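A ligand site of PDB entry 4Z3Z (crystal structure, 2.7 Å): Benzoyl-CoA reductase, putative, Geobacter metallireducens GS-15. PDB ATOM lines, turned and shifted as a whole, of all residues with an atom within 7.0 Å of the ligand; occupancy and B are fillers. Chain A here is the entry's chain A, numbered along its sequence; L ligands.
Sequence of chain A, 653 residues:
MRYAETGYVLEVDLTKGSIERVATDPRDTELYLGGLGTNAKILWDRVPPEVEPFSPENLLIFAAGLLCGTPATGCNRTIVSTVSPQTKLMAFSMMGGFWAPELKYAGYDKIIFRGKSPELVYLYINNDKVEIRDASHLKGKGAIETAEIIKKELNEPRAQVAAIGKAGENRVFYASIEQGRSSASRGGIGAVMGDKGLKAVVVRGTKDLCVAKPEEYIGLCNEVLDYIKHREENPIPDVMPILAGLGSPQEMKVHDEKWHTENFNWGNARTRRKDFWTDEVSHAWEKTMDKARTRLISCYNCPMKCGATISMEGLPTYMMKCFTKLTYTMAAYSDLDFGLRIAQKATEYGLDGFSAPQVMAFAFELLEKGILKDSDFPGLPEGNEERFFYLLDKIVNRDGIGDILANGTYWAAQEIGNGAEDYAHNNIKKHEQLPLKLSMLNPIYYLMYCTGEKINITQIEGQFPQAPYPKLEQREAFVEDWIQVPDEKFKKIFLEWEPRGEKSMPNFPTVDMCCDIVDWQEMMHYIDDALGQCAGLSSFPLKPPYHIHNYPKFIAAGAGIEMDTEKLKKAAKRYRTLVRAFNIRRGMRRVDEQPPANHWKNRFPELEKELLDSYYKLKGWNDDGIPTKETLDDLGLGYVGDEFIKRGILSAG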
ATOM      1  N   THR A  73      -2.808 -34.339  23.299  1.00  0.00           N
ATOM      2  CA  THR A  73      -3.336 -33.543  22.193  1.00  0.00           C
ATOM      3  C   THR A  73      -2.257 -32.762  21.443  1.00  0.00           C
ATOM      4  O   THR A  73      -1.547 -31.950  22.044  1.00  0.00           O
ATOM      5  CB  THR A  73      -4.400 -32.544  22.688  1.00  0.00           C
ATOM      6  OG1 THR A  73      -5.418 -33.242  23.404  1.00  0.00           O
ATOM      7  CG2 THR A  73      -5.020 -31.816  21.511  1.00  0.00           C
ATOM      8  N   GLY A  74      -2.134 -33.007  20.147  1.00  0.00           N
ATOM      9  CA  GLY A  74      -1.254 -32.231  19.300  1.00  0.00           C
ATOM     10  C   GLY A  74       0.169 -32.747  19.204  1.00  0.00           C
ATOM     11  O   GLY A  74       0.936 -32.308  18.349  1.00  0.00           O
ATOM     12  N   CYS A  75       0.530 -33.677  20.083  1.00  0.00           N
ATOM     13  CA  CYS A  75       1.866 -34.232  20.077  1.00  0.00           C
ATOM     14  C   CYS A  75       2.026 -35.238  18.935  1.00  0.00           C
ATOM     15  O   CYS A  75       1.724 -36.420  19.086  1.00  0.00           O
ATOM     16  CB  CYS A  75       2.189 -34.894  21.411  1.00  0.00           C
ATOM     17  SG  CYS A  75       3.934 -35.313  21.624  1.00  0.00           S
ATOM     18  N   ASN A  76       2.524 -34.763  17.800  1.00  0.00           N
ATOM     19  CA  ASN A  76       2.570 -35.564  16.586  1.00  0.00           C
ATOM     20  C   ASN A  76       3.699 -35.188  15.628  1.00  0.00           C
ATOM     21  O   ASN A  76       3.749 -35.672  14.494  1.00  0.00           O
ATOM     22  CB  ASN A  76       1.231 -35.437  15.846  1.00  0.00           C
ATOM     23  CG  ASN A  76       0.812 -33.993  15.653  1.00  0.00           C
ATOM     24  OD1 ASN A  76       1.653 -33.107  15.490  1.00  0.00           O
ATOM     25  ND2 ASN A  76      -0.491 -33.744  15.695  1.00  0.00           N
ATOM     26  N   ARG A  77       4.611 -34.334  16.085  1.00  0.00           N
ATOM     27  CA  ARG A  77       5.637 -33.778  15.209  1.00  0.00           C
ATOM     28  C   ARG A  77       6.777 -34.759  14.919  1.00  0.00           C
ATOM     29  O   ARG A  77       7.170 -35.552  15.761  1.00  0.00           O
ATOM     30  CB  ARG A  77       6.202 -32.490  15.813  1.00  0.00           C
ATOM     31  CG  ARG A  77       5.836 -31.243  15.035  1.00  0.00           C
ATOM     32  CD  ARG A  77       4.327 -31.005  15.017  1.00  0.00           C
ATOM     33  NE  ARG A  77       3.927 -30.075  13.977  1.00  0.00           N
ATOM     34  CZ  ARG A  77       2.662 -29.718  13.730  1.00  0.00           C
ATOM     35  NH1 ARG A  77       1.682 -30.224  14.474  1.00  0.00           N
ATOM     36  NH2 ARG A  77       2.378 -28.861  12.767  1.00  0.00           N
ATOM     37  N   GLY A  96       4.398 -31.754  10.747  1.00  0.00           N
ATOM     38  CA  GLY A  96       3.276 -32.231  11.540  1.00  0.00           C
ATOM     39  C   GLY A  96       2.587 -33.429  10.912  1.00  0.00           C
ATOM     40  O   GLY A  96       3.226 -34.275  10.294  1.00  0.00           O
ATOM     41  N   GLY A  97       1.270 -33.490  11.073  1.00  0.00           N
ATOM     42  CA  GLY A  97       0.489 -34.504  10.392  1.00  0.00           C
ATOM     43  C   GLY A  97       0.313 -35.799  11.142  1.00  0.00           C
ATOM     44  O   GLY A  97      -0.147 -35.805  12.282  1.00  0.00           O
ATOM     45  N   ARG A 181      -0.701 -32.793   4.658  1.00  0.00           N
ATOM     46  CA  ARG A 181      -0.799 -31.365   4.941  1.00  0.00           C
ATOM     47  C   ARG A 181       0.396 -30.868   5.735  1.00  0.00           C
ATOM     48  O   ARG A 181       0.316 -29.843   6.416  1.00  0.00           O
ATOM     49  CB  ARG A 181      -2.095 -31.049   5.691  1.00  0.00           C
ATOM     50  CG  ARG A 181      -2.214 -31.745   7.047  1.00  0.00           C
ATOM     51  CD  ARG A 181      -2.817 -30.822   8.109  1.00  0.00           C
ATOM     52  NE  ARG A 181      -1.886 -29.775   8.513  1.00  0.00           N
ATOM     53  CZ  ARG A 181      -2.091 -28.910   9.497  1.00  0.00           C
ATOM     54  NH1 ARG A 181      -3.216 -28.957  10.211  1.00  0.00           N
ATOM     55  NH2 ARG A 181      -1.184 -27.988   9.787  1.00  0.00           N
ATOM     56  N   SER A 182       1.509 -31.585   5.658  1.00  0.00           N
ATOM     57  CA  SER A 182       2.643 -31.292   6.531  1.00  0.00           C
ATOM     58  C   SER A 182       3.971 -31.258   5.795  1.00  0.00           C
ATOM     59  O   SER A 182       4.198 -32.049   4.882  1.00  0.00           O
ATOM     60  CB  SER A 182       2.685 -32.323   7.653  1.00  0.00           C
ATOM     61  OG  SER A 182       1.450 -32.339   8.345  1.00  0.00           O
ATOM     62  N   LEU A 246      -5.179 -20.241  19.838  1.00  0.00           N
ATOM     63  CA  LEU A 246      -4.184 -21.307  19.818  1.00  0.00           C
ATOM     64  C   LEU A 246      -3.909 -21.796  18.404  1.00  0.00           C
ATOM     65  O   LEU A 246      -4.615 -21.441  17.462  1.00  0.00           O
ATOM     66  CB  LEU A 246      -4.639 -22.480  20.698  1.00  0.00           C
ATOM     67  CG  LEU A 246      -4.807 -22.177  22.183  1.00  0.00           C
ATOM     68  CD1 LEU A 246      -5.279 -23.412  22.926  1.00  0.00           C
ATOM     69  CD2 LEU A 246      -3.511 -21.644  22.766  1.00  0.00           C
ATOM     70  N   GLY A 247      -2.868 -22.615  18.270  1.00  0.00           N
ATOM     71  CA  GLY A 247      -2.493 -23.183  16.989  1.00  0.00           C
ATOM     72  C   GLY A 247      -1.508 -22.334  16.214  1.00  0.00           C
ATOM     73  O   GLY A 247      -1.142 -21.239  16.633  1.00  0.00           O
ATOM     74  N   SER A 248      -1.058 -22.872  15.080  1.00  0.00           N
ATOM     75  CA  SER A 248      -0.281 -22.113  14.105  1.00  0.00           C
ATOM     76  C   SER A 248      -1.073 -20.895  13.664  1.00  0.00           C
ATOM     77  O   SER A 248      -2.304 -20.883  13.802  1.00  0.00           O
ATOM     78  CB  SER A 248       0.070 -23.000  12.915  1.00  0.00           C
ATOM     79  OG  SER A 248       0.595 -24.248  13.328  1.00  0.00           O
ATOM     80  N   GLN A 250      -3.468 -18.778  12.194  1.00  0.00           N
ATOM     81  CA  GLN A 250      -4.675 -19.151  11.461  1.00  0.00           C
ATOM     82  C   GLN A 250      -4.851 -18.326  10.190  1.00  0.00           C
ATOM     83  O   GLN A 250      -5.810 -17.575  10.054  1.00  0.00           O
ATOM     84  CB  GLN A 250      -5.899 -18.998  12.368  1.00  0.00           C
ATOM     85  CG  GLN A 250      -5.817 -19.779  13.667  1.00  0.00           C
ATOM     86  CD  GLN A 250      -5.915 -21.277  13.470  1.00  0.00           C
ATOM     87  OE1 GLN A 250      -6.138 -21.764  12.354  1.00  0.00           O
ATOM     88  NE2 GLN A 250      -5.744 -22.029  14.545  1.00  0.00           N
ATOM     89  N   ILE A 297      -8.570 -28.554   8.033  1.00  0.00           N
ATOM     90  CA  ILE A 297      -8.234 -29.858   8.601  1.00  0.00           C
ATOM     91  C   ILE A 297      -7.106 -29.802   9.620  1.00  0.00           C
ATOM     92  O   ILE A 297      -6.315 -28.847   9.658  1.00  0.00           O
ATOM     93  CB  ILE A 297      -7.837 -30.855   7.494  1.00  0.00           C
ATOM     94  CG1 ILE A 297      -6.647 -30.320   6.701  1.00  0.00           C
ATOM     95  CG2 ILE A 297      -9.035 -31.115   6.575  1.00  0.00           C
ATOM     96  CD1 ILE A 297      -6.130 -31.301   5.681  1.00  0.00           C
ATOM     97  N   SER A 298      -7.031 -30.849  10.445  1.00  0.00           N
ATOM     98  CA  SER A 298      -6.116 -30.920  11.576  1.00  0.00           C
ATOM     99  C   SER A 298      -4.958 -31.879  11.371  1.00  0.00           C
ATOM    100  O   SER A 298      -4.968 -32.705  10.462  1.00  0.00           O
ATOM    101  CB  SER A 298      -6.858 -31.349  12.833  1.00  0.00           C
ATOM    102  OG  SER A 298      -7.813 -30.387  13.242  1.00  0.00           O
ATOM    103  N   CYS A 299      -3.962 -31.779  12.243  1.00  0.00           N
ATOM    104  CA  CYS A 299      -2.947 -32.813  12.371  1.00  0.00           C
ATOM    105  C   CYS A 299      -3.521 -33.897  13.279  1.00  0.00           C
ATOM    106  O   CYS A 299      -4.650 -33.790  13.757  1.00  0.00           O
ATOM    107  CB  CYS A 299      -1.641 -32.246  12.944  1.00  0.00           C
ATOM    108  SG  CYS A 299      -0.981 -30.800  12.068  1.00  0.00           S
ATOM    109  N   TYR A 300      -2.742 -34.944  13.538  1.00  0.00           N
ATOM    110  CA  TYR A 300      -3.170 -36.029  14.423  1.00  0.00           C
ATOM    111  C   TYR A 300      -3.589 -35.536  15.802  1.00  0.00           C
ATOM    112  O   TYR A 300      -2.880 -34.764  16.423  1.00  0.00           O
ATOM    113  CB  TYR A 300      -2.045 -37.054  14.553  1.00  0.00           C
ATOM    114  CG  TYR A 300      -2.441 -38.360  15.213  1.00  0.00           C
ATOM    115  CD1 TYR A 300      -3.335 -39.223  14.594  1.00  0.00           C
ATOM    116  CD2 TYR A 300      -1.878 -38.746  16.425  1.00  0.00           C
ATOM    117  CE1 TYR A 300      -3.684 -40.426  15.180  1.00  0.00           C
ATOM    118  CE2 TYR A 300      -2.217 -39.954  17.019  1.00  0.00           C
ATOM    119  CZ  TYR A 300      -3.122 -40.790  16.396  1.00  0.00           C
ATOM    120  OH  TYR A 300      -3.457 -41.988  16.982  1.00  0.00           O
ATOM    121  N   ASN A 301      -4.766 -35.972  16.248  1.00  0.00           N
ATOM    122  CA  ASN A 301      -5.236 -35.739  17.614  1.00  0.00           C
ATOM    123  C   ASN A 301      -5.229 -34.262  18.020  1.00  0.00           C
ATOM    124  O   ASN A 301      -4.667 -33.899  19.055  1.00  0.00           O
ATOM    125  CB  ASN A 301      -4.368 -36.557  18.588  1.00  0.00           C
ATOM    126  CG  ASN A 301      -4.965 -36.627  19.983  1.00  0.00           C
ATOM    127  OD1 ASN A 301      -6.111 -36.233  20.213  1.00  0.00           O
ATOM    128  ND2 ASN A 301      -4.190 -37.162  20.926  1.00  0.00           N
ATOM    129  N   CYS A 302      -5.844 -33.407  17.207  1.00  0.00           N
ATOM    130  CA  CYS A 302      -5.928 -31.980  17.519  1.00  0.00           C
ATOM    131  C   CYS A 302      -7.185 -31.353  16.929  1.00  0.00           C
ATOM    132  O   CYS A 302      -7.553 -31.638  15.794  1.00  0.00           O
ATOM    133  CB  CYS A 302      -4.688 -31.250  17.005  1.00  0.00           C
ATOM    134  SG  CYS A 302      -4.642 -29.479  17.405  1.00  0.00           S
ATOM    135  N   PRO A 303      -7.854 -30.483  17.698  1.00  0.00           N
ATOM    136  CA  PRO A 303      -9.097 -29.847  17.258  1.00  0.00           C
ATOM    137  C   PRO A 303      -8.932 -28.459  16.639  1.00  0.00           C
ATOM    138  O   PRO A 303      -9.939 -27.803  16.368  1.00  0.00           O
ATOM    139  CB  PRO A 303      -9.889 -29.735  18.561  1.00  0.00           C
ATOM    140  CG  PRO A 303      -8.831 -29.458  19.573  1.00  0.00           C
ATOM    141  CD  PRO A 303      -7.607 -30.247  19.136  1.00  0.00           C
ATOM    142  N   MET A 304      -7.698 -28.018  16.420  1.00  0.00           N
ATOM    143  CA  MET A 304      -7.459 -26.646  15.995  1.00  0.00           C
ATOM    144  C   MET A 304      -7.614 -26.423  14.498  1.00  0.00           C
ATOM    145  O   MET A 304      -7.845 -25.285  14.062  1.00  0.00           O
ATOM    146  CB  MET A 304      -6.064 -26.197  16.427  1.00  0.00           C
ATOM    147  CG  MET A 304      -5.865 -26.141  17.935  1.00  0.00           C
ATOM    148  SD  MET A 304      -7.183 -25.226  18.761  1.00  0.00           S
ATOM    149  CE  MET A 304      -7.087 -23.653  17.917  1.00  0.00           C
ATOM    150  N   LYS A 305      -7.518 -27.499  13.732  1.00  0.00           N
ATOM    151  CA  LYS A 305      -7.616 -27.489  12.261  1.00  0.00           C
ATOM    152  C   LYS A 305      -7.015 -26.244  11.614  1.00  0.00           C
ATOM    153  O   LYS A 305      -7.728 -25.434  11.013  1.00  0.00           O
ATOM    154  CB  LYS A 305      -9.085 -27.664  11.815  1.00  0.00           C
ATOM    155  CG  LYS A 305     -10.108 -26.750  12.482  1.00  0.00           C
ATOM    156  CD  LYS A 305     -11.524 -27.170  12.137  1.00  0.00           C
ATOM    157  CE  LYS A 305     -12.542 -26.383  12.944  1.00  0.00           C
ATOM    158  NZ  LYS A 305     -13.922 -26.870  12.697  1.00  0.00           N
ATOM    159  N   CYS A 306      -5.712 -26.118  11.751  1.00  0.00           N
ATOM    160  CA  CYS A 306      -4.988 -24.970  11.214  1.00  0.00           C
ATOM    161  C   CYS A 306      -4.770 -25.126   9.714  1.00  0.00           C
ATOM    162  O   CYS A 306      -4.621 -24.140   8.996  1.00  0.00           O
ATOM    163  CB  CYS A 306      -3.650 -24.798  11.935  1.00  0.00           C
ATOM    164  SG  CYS A 306      -3.775 -24.795  13.735  1.00  0.00           S
ATOM    165  N   GLY A 307      -4.772 -26.373   9.249  1.00  0.00           N
ATOM    166  CA  GLY A 307      -4.531 -26.636   7.837  1.00  0.00           C
ATOM    167  C   GLY A 307      -5.760 -26.409   6.987  1.00  0.00           C
ATOM    168  O   GLY A 307      -6.864 -26.254   7.504  1.00  0.00           O
ATOM    169  N   LYS A 321      -0.921 -24.287   5.096  1.00  0.00           N
ATOM    170  CA  LYS A 321      -1.093 -23.639   6.392  1.00  0.00           C
ATOM    171  C   LYS A 321      -0.150 -22.439   6.519  1.00  0.00           C
ATOM    172  O   LYS A 321       0.794 -22.309   5.735  1.00  0.00           O
ATOM    173  CB  LYS A 321      -0.847 -24.633   7.533  1.00  0.00           C
ATOM    174  CG  LYS A 321       0.585 -24.721   8.040  1.00  0.00           C
ATOM    175  CD  LYS A 321       1.549 -25.288   6.992  1.00  0.00           C
ATOM    176  CE  LYS A 321       1.209 -26.711   6.627  1.00  0.00           C
ATOM    177  NZ  LYS A 321       2.162 -27.272   5.641  1.00  0.00           N
ATOM    178  N   GLN A 533       5.684 -32.428  20.613  1.00  0.00           N
ATOM    179  CA  GLN A 533       4.477 -31.633  20.786  1.00  0.00           C
ATOM    180  C   GLN A 533       4.427 -30.476  19.790  1.00  0.00           C
ATOM    181  O   GLN A 533       5.428 -29.801  19.555  1.00  0.00           O
ATOM    182  CB  GLN A 533       4.397 -31.101  22.212  1.00  0.00           C
ATOM    183  CG  GLN A 533       3.247 -30.146  22.440  1.00  0.00           C
ATOM    184  CD  GLN A 533       1.903 -30.808  22.234  1.00  0.00           C
ATOM    185  OE1 GLN A 533       1.681 -31.932  22.678  1.00  0.00           O
ATOM    186  NE2 GLN A 533       0.996 -30.116  21.559  1.00  0.00           N
ATOM    187  N   CYS A 534       3.252 -30.238  19.209  1.00  0.00           N
ATOM    188  CA  CYS A 534       3.093 -29.136  18.261  1.00  0.00           C
ATOM    189  C   CYS A 534       3.185 -27.794  18.965  1.00  0.00           C
ATOM    190  O   CYS A 534       2.521 -27.572  19.986  1.00  0.00           O
ATOM    191  CB  CYS A 534       1.771 -29.230  17.516  1.00  0.00           C
ATOM    192  SG  CYS A 534       1.531 -27.895  16.330  1.00  0.00           S
ATOM    193  N   ALA A 535       3.992 -26.899  18.412  1.00  0.00           N
ATOM    194  CA  ALA A 535       4.186 -25.572  18.984  1.00  0.00           C
ATOM    195  C   ALA A 535       2.881 -24.789  19.049  1.00  0.00           C
ATOM    196  O   ALA A 535       2.756 -23.853  19.823  1.00  0.00           O
ATOM    197  CB  ALA A 535       5.214 -24.810  18.174  1.00  0.00           C
ATOM    198  N   GLY A 536       1.910 -25.195  18.234  1.00  0.00           N
ATOM    199  CA  GLY A 536       0.608 -24.547  18.195  1.00  0.00           C
ATOM    200  C   GLY A 536      -0.170 -24.648  19.492  1.00  0.00           C
ATOM    201  O   GLY A 536      -1.097 -23.878  19.721  1.00  0.00           O
ATOM    202  N   LEU A 537       0.213 -25.594  20.346  1.00  0.00           N
ATOM    203  CA  LEU A 537      -0.439 -25.745  21.632  1.00  0.00           C
ATOM    204  C   LEU A 537       0.534 -25.477  22.787  1.00  0.00           C
ATOM    205  O   LEU A 537       0.221 -25.749  23.948  1.00  0.00           O
ATOM    206  CB  LEU A 537      -1.045 -27.141  21.776  1.00  0.00           C
ATOM    207  CG  LEU A 537      -2.150 -27.497  20.785  1.00  0.00           C
ATOM    208  CD1 LEU A 537      -2.699 -28.878  21.082  1.00  0.00           C
ATOM    209  CD2 LEU A 537      -3.253 -26.448  20.818  1.00  0.00           C
HETATM  210 FE1  LIG L   1      -1.505 -29.019  13.554  1.00  0.00          FE
HETATM  211 FE2  LIG L   1      -3.061 -28.915  15.834  1.00  0.00          FE
HETATM  212 FE3  LIG L   1      -2.739 -26.687  14.380  1.00  0.00          FE
HETATM  213 FE4  LIG L   1      -0.693 -27.637  15.786  1.00  0.00          FE
HETATM  214  S1  LIG L   1      -2.637 -26.815  16.690  1.00  0.00           S
HETATM  215  S2  LIG L   1      -0.586 -26.921  13.603  1.00  0.00           S
HETATM  216  S3  LIG L   1      -1.011 -29.921  15.594  1.00  0.00           S
HETATM  217  S4  LIG L   1      -3.772 -28.616  13.653  1.00  0.00           S
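The side-chain sulfur (SG) of Cys 306 lies close to the backbone NH (N) of Ser 248, at 3.6 Å. N of Gly 536 lies close to SG of Cys 534 (3.3 Å). The side-chain amide nitrogen (ND2) of Asn 76 lies within hydrogen-bond range of the backbone carbonyl oxygen (O) of Tyr 300, 2.7 Å away. N of Lys 305 is in hydrogen-bond range of OG of Ser 298. The guanidinium group (NH1) of Arg 77 lies close to the side-chain sulfur (SG) of Cys 299, at 3.6 Å. The backbone carbonyl oxygen (O) of Arg 181 is in hydrogen-bond range of the side-chain amino group (NZ) of Lys 321 (3.3 Å). The backbone carbonyl oxygen (O) of Gly 74 is in hydrogen-bond range of the backbone NH (N) of Cys 534, 3.2 Å away. NH1 of Arg 77 lies close to SG of Cys 534 (3.0 Å).
A sulfur (S4) of the ligand sits close to the backbone NH of Cys 299. N of Cys 306 lies close to S4 of the ligand, 3.7 Å away. A sulfur (S3) of the ligand lies close to the guanidinium group (NH1) of Arg 77 (2.9 Å). FE2 of the ligand is bound by SG of Cys 302 (2.3 Å). SG of Cys 299 binds FE1 of the ligand. SG of Cys 306 is bound to FE3 of the ligand (2.3 Å). S2 of the ligand sits close to OG of Ser 248 (2.9 Å). The guanidinium group (NH1) of Arg 181 lies close to a sulfur (S4) of the ligand. SG of Cys 534 binds FE4 of the ligand, 2.3 Å away.
Asn 76 touches the ligand. CA of Gly 247 touches S1 of the ligand, 3.6 Å away. CA of Ser 298 touches S4 of the ligand, 3.9 Å away. Met 304 touches the ligand. Lys 305 touches the ligand (N to S4, 3.9 Å). Hydrophobic or aromatic side chains that line the ligand: Met 304. Of the 30 residues printed, 12 come within 4 Å of the ligand. The nearest printed residue that does not touch the ligand is Gly 536 (4.1 Å).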
